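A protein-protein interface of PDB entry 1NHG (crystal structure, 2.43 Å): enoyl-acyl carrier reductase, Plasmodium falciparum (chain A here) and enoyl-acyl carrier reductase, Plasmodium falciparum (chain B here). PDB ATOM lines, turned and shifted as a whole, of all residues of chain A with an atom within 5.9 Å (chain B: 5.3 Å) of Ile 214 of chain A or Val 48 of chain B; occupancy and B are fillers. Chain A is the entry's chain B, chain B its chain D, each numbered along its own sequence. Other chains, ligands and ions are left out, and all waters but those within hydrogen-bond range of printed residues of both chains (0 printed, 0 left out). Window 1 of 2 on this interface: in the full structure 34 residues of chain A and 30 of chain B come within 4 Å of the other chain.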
ATOM      1  N   TYR A  15      -4.471  -2.650   6.345  1.00  0.00           N
ATOM      2  CA  TYR A  15      -3.636  -1.459   6.403  1.00  0.00           C
ATOM      3  C   TYR A  15      -2.623  -1.534   7.526  1.00  0.00           C
ATOM      4  O   TYR A  15      -1.554  -0.933   7.448  1.00  0.00           O
ATOM      5  CB  TYR A  15      -4.501  -0.209   6.561  1.00  0.00           C
ATOM      6  CG  TYR A  15      -5.081   0.288   5.257  1.00  0.00           C
ATOM      7  CD1 TYR A  15      -4.256   0.585   4.182  1.00  0.00           C
ATOM      8  CD2 TYR A  15      -6.452   0.494   5.112  1.00  0.00           C
ATOM      9  CE1 TYR A  15      -4.775   1.081   2.992  1.00  0.00           C
ATOM     10  CE2 TYR A  15      -6.979   0.991   3.930  1.00  0.00           C
ATOM     11  CZ  TYR A  15      -6.136   1.284   2.875  1.00  0.00           C
ATOM     12  OH  TYR A  15      -6.651   1.799   1.710  1.00  0.00           O
ATOM     13  N   ILE A 167      -2.015   7.781  15.483  1.00  0.00           N
ATOM     14  CA  ILE A 167      -2.875   7.856  14.299  1.00  0.00           C
ATOM     15  C   ILE A 167      -3.892   6.726  14.296  1.00  0.00           C
ATOM     16  O   ILE A 167      -3.686   5.682  14.915  1.00  0.00           O
ATOM     17  CB  ILE A 167      -2.106   7.747  12.949  1.00  0.00           C
ATOM     18  CG1 ILE A 167      -1.454   6.370  12.836  1.00  0.00           C
ATOM     19  CG2 ILE A 167      -1.123   8.898  12.799  1.00  0.00           C
ATOM     20  CD1 ILE A 167      -0.880   6.064  11.466  1.00  0.00           C
ATOM     21  N   SER A 168      -4.996   6.953  13.594  1.00  0.00           N
ATOM     22  CA  SER A 168      -6.051   5.960  13.442  1.00  0.00           C
ATOM     23  C   SER A 168      -6.491   6.068  11.984  1.00  0.00           C
ATOM     24  O   SER A 168      -6.055   6.974  11.268  1.00  0.00           O
ATOM     25  CB  SER A 168      -7.226   6.264  14.368  1.00  0.00           C
ATOM     26  OG  SER A 168      -7.888   7.441  13.966  1.00  0.00           O
ATOM     27  N   LEU A 169      -7.341   5.146  11.543  1.00  0.00           N
ATOM     28  CA  LEU A 169      -7.825   5.149  10.161  1.00  0.00           C
ATOM     29  C   LEU A 169      -9.333   5.403  10.102  1.00  0.00           C
ATOM     30  O   LEU A 169     -10.100   4.861  10.898  1.00  0.00           O
ATOM     31  CB  LEU A 169      -7.528   3.804   9.480  1.00  0.00           C
ATOM     32  CG  LEU A 169      -6.115   3.284   9.182  1.00  0.00           C
ATOM     33  CD1 LEU A 169      -5.505   4.099   8.068  1.00  0.00           C
ATOM     34  CD2 LEU A 169      -5.257   3.324  10.430  1.00  0.00           C
ATOM     35  N   THR A 170      -9.755   6.226   9.152  1.00  0.00           N
ATOM     36  CA  THR A 170     -11.176   6.509   8.990  1.00  0.00           C
ATOM     37  C   THR A 170     -11.581   6.378   7.519  1.00  0.00           C
ATOM     38  O   THR A 170     -10.771   5.988   6.674  1.00  0.00           O
ATOM     39  CB  THR A 170     -11.530   7.920   9.493  1.00  0.00           C
ATOM     40  OG1 THR A 170     -12.954   8.071   9.480  1.00  0.00           O
ATOM     41  CG2 THR A 170     -10.887   8.992   8.608  1.00  0.00           C
ATOM     42  N   TYR A 171     -12.830   6.710   7.212  1.00  0.00           N
ATOM     43  CA  TYR A 171     -13.328   6.596   5.847  1.00  0.00           C
ATOM     44  C   TYR A 171     -14.305   7.727   5.558  1.00  0.00           C
ATOM     45  O   TYR A 171     -15.043   8.169   6.442  1.00  0.00           O
ATOM     46  CB  TYR A 171     -13.999   5.229   5.651  1.00  0.00           C
ATOM     47  CG  TYR A 171     -14.518   4.961   4.253  1.00  0.00           C
ATOM     48  CD1 TYR A 171     -13.683   5.069   3.138  1.00  0.00           C
ATOM     49  CD2 TYR A 171     -15.854   4.605   4.046  1.00  0.00           C
ATOM     50  CE1 TYR A 171     -14.168   4.834   1.848  1.00  0.00           C
ATOM     51  CE2 TYR A 171     -16.352   4.365   2.761  1.00  0.00           C
ATOM     52  CZ  TYR A 171     -15.508   4.482   1.665  1.00  0.00           C
ATOM     53  OH  TYR A 171     -16.010   4.247   0.400  1.00  0.00           O
ATOM     54  N   ASN A 212      -3.618  12.266  14.809  1.00  0.00           N
ATOM     55  CA  ASN A 212      -4.269  12.576  13.542  1.00  0.00           C
ATOM     56  C   ASN A 212      -4.963  11.324  13.037  1.00  0.00           C
ATOM     57  O   ASN A 212      -4.751  10.225  13.563  1.00  0.00           O
ATOM     58  CB  ASN A 212      -3.244  13.039  12.507  1.00  0.00           C
ATOM     59  CG  ASN A 212      -2.627  14.386  12.851  1.00  0.00           C
ATOM     60  OD1 ASN A 212      -3.244  15.439  12.663  1.00  0.00           O
ATOM     61  ND2 ASN A 212      -1.407  14.357  13.374  1.00  0.00           N
ATOM     62  N   THR A 213      -5.801  11.478  12.023  1.00  0.00           N
ATOM     63  CA  THR A 213      -6.475  10.313  11.489  1.00  0.00           C
ATOM     64  C   THR A 213      -6.373  10.314   9.973  1.00  0.00           C
ATOM     65  O   THR A 213      -6.485  11.358   9.327  1.00  0.00           O
ATOM     66  CB  THR A 213      -7.948  10.258  11.950  1.00  0.00           C
ATOM     67  OG1 THR A 213      -8.507   9.004  11.556  1.00  0.00           O
ATOM     68  CG2 THR A 213      -8.763  11.401  11.353  1.00  0.00           C
ATOM     69  N   ILE A 214      -6.114   9.141   9.412  1.00  0.00           N
ATOM     70  CA  ILE A 214      -5.974   8.987   7.975  1.00  0.00           C
ATOM     71  C   ILE A 214      -7.243   8.420   7.351  1.00  0.00           C
ATOM     72  O   ILE A 214      -7.687   7.333   7.719  1.00  0.00           O
ATOM     73  CB  ILE A 214      -4.800   8.043   7.647  1.00  0.00           C
ATOM     74  CG1 ILE A 214      -3.484   8.683   8.086  1.00  0.00           C
ATOM     75  CG2 ILE A 214      -4.770   7.731   6.155  1.00  0.00           C
ATOM     76  CD1 ILE A 214      -2.272   7.795   7.860  1.00  0.00           C
ATOM     77  N   SER A 215      -7.829   9.161   6.416  1.00  0.00           N
ATOM     78  CA  SER A 215      -9.034   8.704   5.727  1.00  0.00           C
ATOM     79  C   SER A 215      -8.524   7.980   4.481  1.00  0.00           C
ATOM     80  O   SER A 215      -8.110   8.615   3.507  1.00  0.00           O
ATOM     81  CB  SER A 215      -9.909   9.895   5.337  1.00  0.00           C
ATOM     82  OG  SER A 215     -11.185   9.471   4.897  1.00  0.00           O
ATOM     83  N   ALA A 216      -8.550   6.651   4.519  1.00  0.00           N
ATOM     84  CA  ALA A 216      -8.033   5.851   3.416  1.00  0.00           C
ATOM     85  C   ALA A 216      -9.023   5.490   2.327  1.00  0.00           C
ATOM     86  O   ALA A 216     -10.229   5.461   2.546  1.00  0.00           O
ATOM     87  CB  ALA A 216      -7.408   4.581   3.960  1.00  0.00           C
ATOM     88  N   GLY A 217      -8.484   5.209   1.146  1.00  0.00           N
ATOM     89  CA  GLY A 217      -9.314   4.806   0.030  1.00  0.00           C
ATOM     90  C   GLY A 217      -9.642   3.327   0.179  1.00  0.00           C
ATOM     91  O   GLY A 217      -9.288   2.711   1.190  1.00  0.00           O
ATOM     92  N   LEU B  21      -4.482   1.652  -5.288  1.00  0.00           N
ATOM     93  CA  LEU B  21      -4.126   2.135  -3.963  1.00  0.00           C
ATOM     94  C   LEU B  21      -3.586   0.956  -3.178  1.00  0.00           C
ATOM     95  O   LEU B  21      -4.298  -0.016  -2.950  1.00  0.00           O
ATOM     96  CB  LEU B  21      -5.353   2.710  -3.257  1.00  0.00           C
ATOM     97  CG  LEU B  21      -5.094   3.298  -1.873  1.00  0.00           C
ATOM     98  CD1 LEU B  21      -4.128   4.471  -1.978  1.00  0.00           C
ATOM     99  CD2 LEU B  21      -6.412   3.739  -1.261  1.00  0.00           C
ATOM    100  N   ASP B  25       0.793   2.549   0.588  1.00  0.00           N
ATOM    101  CA  ASP B  25       0.628   3.955   0.208  1.00  0.00           C
ATOM    102  C   ASP B  25       0.157   4.687   1.457  1.00  0.00           C
ATOM    103  O   ASP B  25       0.536   5.828   1.712  1.00  0.00           O
ATOM    104  CB  ASP B  25      -0.426   4.136  -0.891  1.00  0.00           C
ATOM    105  CG  ASP B  25       0.099   3.789  -2.270  1.00  0.00           C
ATOM    106  OD1 ASP B  25       1.322   3.926  -2.504  1.00  0.00           O
ATOM    107  OD2 ASP B  25      -0.722   3.396  -3.126  1.00  0.00           O
ATOM    108  N   ILE B  26      -0.681   4.013   2.234  1.00  0.00           N
ATOM    109  CA  ILE B  26      -1.187   4.578   3.469  1.00  0.00           C
ATOM    110  C   ILE B  26      -0.068   4.452   4.504  1.00  0.00           C
ATOM    111  O   ILE B  26       0.138   5.348   5.333  1.00  0.00           O
ATOM    112  CB  ILE B  26      -2.452   3.814   3.946  1.00  0.00           C
ATOM    113  CG1 ILE B  26      -3.702   4.404   3.282  1.00  0.00           C
ATOM    114  CG2 ILE B  26      -2.563   3.870   5.461  1.00  0.00           C
ATOM    115  CD1 ILE B  26      -3.694   4.388   1.753  1.00  0.00           C
ATOM    116  N   VAL B  29       2.463   7.314   4.378  1.00  0.00           N
ATOM    117  CA  VAL B  29       1.872   8.539   4.902  1.00  0.00           C
ATOM    118  C   VAL B  29       1.749   8.385   6.416  1.00  0.00           C
ATOM    119  O   VAL B  29       1.964   9.336   7.163  1.00  0.00           O
ATOM    120  CB  VAL B  29       0.479   8.807   4.285  1.00  0.00           C
ATOM    121  CG1 VAL B  29      -0.143  10.055   4.913  1.00  0.00           C
ATOM    122  CG2 VAL B  29       0.609   8.984   2.788  1.00  0.00           C
ATOM    123  N   ALA B  30       1.421   7.176   6.868  1.00  0.00           N
ATOM    124  CA  ALA B  30       1.291   6.902   8.300  1.00  0.00           C
ATOM    125  C   ALA B  30       2.652   7.070   8.963  1.00  0.00           C
ATOM    126  O   ALA B  30       2.770   7.576  10.078  1.00  0.00           O
ATOM    127  CB  ALA B  30       0.785   5.482   8.521  1.00  0.00           C
ATOM    128  N   LEU B  33       3.386  10.845   9.464  1.00  0.00           N
ATOM    129  CA  LEU B  33       2.629  11.473  10.547  1.00  0.00           C
ATOM    130  C   LEU B  33       3.120  11.046  11.930  1.00  0.00           C
ATOM    131  O   LEU B  33       3.014  11.811  12.890  1.00  0.00           O
ATOM    132  CB  LEU B  33       1.131  11.171  10.402  1.00  0.00           C
ATOM    133  CG  LEU B  33       0.389  11.946   9.302  1.00  0.00           C
ATOM    134  CD1 LEU B  33      -0.952  11.303   9.018  1.00  0.00           C
ATOM    135  CD2 LEU B  33       0.208  13.389   9.736  1.00  0.00           C
ATOM    136  N   ILE B  46      -6.324  13.405   7.323  1.00  0.00           N
ATOM    137  CA  ILE B  46      -5.568  13.459   6.077  1.00  0.00           C
ATOM    138  C   ILE B  46      -6.085  12.398   5.111  1.00  0.00           C
ATOM    139  O   ILE B  46      -6.132  11.210   5.437  1.00  0.00           O
ATOM    140  CB  ILE B  46      -4.058  13.203   6.315  1.00  0.00           C
ATOM    141  CG1 ILE B  46      -3.541  14.066   7.472  1.00  0.00           C
ATOM    142  CG2 ILE B  46      -3.280  13.498   5.039  1.00  0.00           C
ATOM    143  CD1 ILE B  46      -3.569  15.551   7.209  1.00  0.00           C
ATOM    144  N   TYR B  47      -6.467  12.841   3.921  1.00  0.00           N
ATOM    145  CA  TYR B  47      -6.981  11.958   2.890  1.00  0.00           C
ATOM    146  C   TYR B  47      -5.878  11.340   2.030  1.00  0.00           C
ATOM    147  O   TYR B  47      -5.079  12.052   1.423  1.00  0.00           O
ATOM    148  CB  TYR B  47      -7.961  12.734   1.999  1.00  0.00           C
ATOM    149  CG  TYR B  47      -9.354  12.839   2.582  1.00  0.00           C
ATOM    150  CD1 TYR B  47     -10.314  11.863   2.314  1.00  0.00           C
ATOM    151  CD2 TYR B  47      -9.703  13.888   3.434  1.00  0.00           C
ATOM    152  CE1 TYR B  47     -11.583  11.927   2.875  1.00  0.00           C
ATOM    153  CE2 TYR B  47     -10.979  13.959   4.003  1.00  0.00           C
ATOM    154  CZ  TYR B  47     -11.911  12.974   3.718  1.00  0.00           C
ATOM    155  OH  TYR B  47     -13.178  13.023   4.263  1.00  0.00           O
ATOM    156  N   VAL B  48      -5.838  10.009   2.011  1.00  0.00           N
ATOM    157  CA  VAL B  48      -4.878   9.232   1.217  1.00  0.00           C
ATOM    158  C   VAL B  48      -5.786   8.305   0.401  1.00  0.00           C
ATOM    159  O   VAL B  48      -6.001   7.136   0.752  1.00  0.00           O
ATOM    160  CB  VAL B  48      -3.950   8.386   2.114  1.00  0.00           C
ATOM    161  CG1 VAL B  48      -2.857   7.772   1.276  1.00  0.00           C
ATOM    162  CG2 VAL B  48      -3.352   9.243   3.211  1.00  0.00           C
ATOM    163  N   ASP B  49      -6.321   8.848  -0.688  1.00  0.00           N
ATOM    164  CA  ASP B  49      -7.271   8.125  -1.514  1.00  0.00           C
ATOM    165  C   ASP B  49      -7.131   8.459  -2.998  1.00  0.00           C
ATOM    166  O   ASP B  49      -8.099   8.381  -3.757  1.00  0.00           O
ATOM    167  CB  ASP B  49      -8.674   8.501  -1.043  1.00  0.00           C
ATOM    168  CG  ASP B  49      -8.983   9.975  -1.274  1.00  0.00           C
ATOM    169  OD1 ASP B  49      -8.045  10.741  -1.611  1.00  0.00           O
ATOM    170  OD2 ASP B  49     -10.161  10.370  -1.122  1.00  0.00           O
ATOM    171  N   ASN B  50      -5.927   8.836  -3.405  1.00  0.00           N
ATOM    172  CA  ASN B  50      -5.668   9.200  -4.792  1.00  0.00           C
ATOM    173  C   ASN B  50      -6.521  10.384  -5.231  1.00  0.00           C
ATOM    174  O   ASN B  50      -6.696  10.626  -6.427  1.00  0.00           O
ATOM    175  CB  ASN B  50      -5.902   8.000  -5.715  1.00  0.00           C
ATOM    176  CG  ASN B  50      -4.854   6.915  -5.525  1.00  0.00           C
ATOM    177  OD1 ASN B  50      -3.668   7.212  -5.351  1.00  0.00           O
ATOM    178  ND2 ASN B  50      -5.281   5.654  -5.569  1.00  0.00           N
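The backbone carbonyl oxygen (O) of Val 48 of chain B sits at hydrogen-bond distance from the backbone NH (N) of Gly 217 of chain A (3.2 Å).
The backbone NH (N) of Ser 215 of chain A is in hydrogen-bond range of the backbone carbonyl oxygen (O) of Ile 46 of chain B.
N of Ile 46 of chain B lies within hydrogen-bond range of O of Thr 213 of chain A.
The backbone carbonyl oxygen (O) of Ser 215 of chain A is in hydrogen-bond range of the backbone NH (N) of Val 48 of chain B, at 3.1 Å.
O of Thr 170 of chain A lies within hydrogen-bond range of N of Ala 216 of chain A (3.2 Å).
The side-chain hydroxyl of Thr 213 of chain A is in hydrogen-bond range of the side-chain hydroxyl of Ser 168 of chain A (2.9 Å).
O of Ser 168 of chain A lies within hydrogen-bond range of N of Ile 214 of chain A, 2.9 Å away.
The backbone carbonyl oxygen (O) of Ile 214 of chain A lies within hydrogen-bond range of the backbone NH (N) of Thr 170 of chain A (2.7 Å).
The backbone carbonyl oxygen of Gly 217 of chain A lies within hydrogen-bond range of the side-chain hydroxyl of Tyr 15 of chain A (2.8 Å).
Among the printed residues, merely in contact across the chains: Tyr 15 of chain A with Leu 21 of chain B (3.6 Å), Tyr 15 of chain A with Ile 26 of chain B (3.5 Å), Ile 167 of chain A with Ala 30 of chain B (3.4 Å), Ile 167 of chain A with Leu 33 of chain B (3.999 Å), Leu 169 of chain A with Ile 26 of chain B (3.9 Å), Ile 214 of chain A with Ala 30 of chain B (3.7 Å), Ile 214 of chain A with Leu 33 of chain B (3.8 Å), Ile 214 of chain A with Ile 46 of chain B (3.4 Å), Ile 214 of chain A with Val 48 of chain B (3.6 Å), Ser 215 of chain A with Tyr 47 of chain B (3.2 Å), Ala 216 of chain A with Ile 26 of chain B (3.8 Å), Ala 216 of chain A with Val 48 of chain B (3.6 Å), Gly 217 of chain A with Leu 21 of chain B (3.4 Å) and Gly 217 of chain A with Asp 49 of chain B (3.9 Å).
Of chain B, only Ala 30, Leu 33, Ile 46 and Val 48 come within 4 Å of Ile 214 of chain A.
Of the printed residues of chain A, Ile 46 of chain B touches Thr 213, Ile 214 and Ser 215.
Of the printed residues of chain A, Tyr 47 of chain B touches Ser 215 (3.2 Å).
Of the printed residues of chain B, Ile 167 of chain A touches Ala 30 (3.4 Å) and Leu 33 (3.999 Å).
Printed residues of chain B within 4 Å of Tyr 15 of chain A: Leu 21 and Ile 26.
Printed residues of chain A within 4 Å of Ile 26 of chain B: Tyr 15, Leu 169 and Ala 216.
Asn 212 of chain A touches none of the printed residues of chain B.
The nearest residue of chain A that does not touch Val 48 of chain B is Tyr 15 of chain A (5.5 Å).
The nearest printed residue of chain A that does not touch Asp 49 of chain B is Ala 216 of chain A (4.5 Å).
Of the 11 printed residues of chain B, 8 touch a printed residue of chain A.
Printed residues of chain B that touch a printed residue of chain A: Leu 21, Ile 26, Ala 30, Leu 33, Ile 46, Tyr 47, Val 48 and Asp 49.
Of the 12 printed residues of chain A, 8 touch a printed residue of chain B.
Hydrophobic or aromatic side chains of chain A within 4 Å of the printed part of chain B: Tyr 15, Ile 167, Leu 169, Ile 214 and Ala 216.
Among the printed residues, no Asp or Glu carboxylate lies within 4 Å of a Lys or Arg side-chain nitrogen of the other chain.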
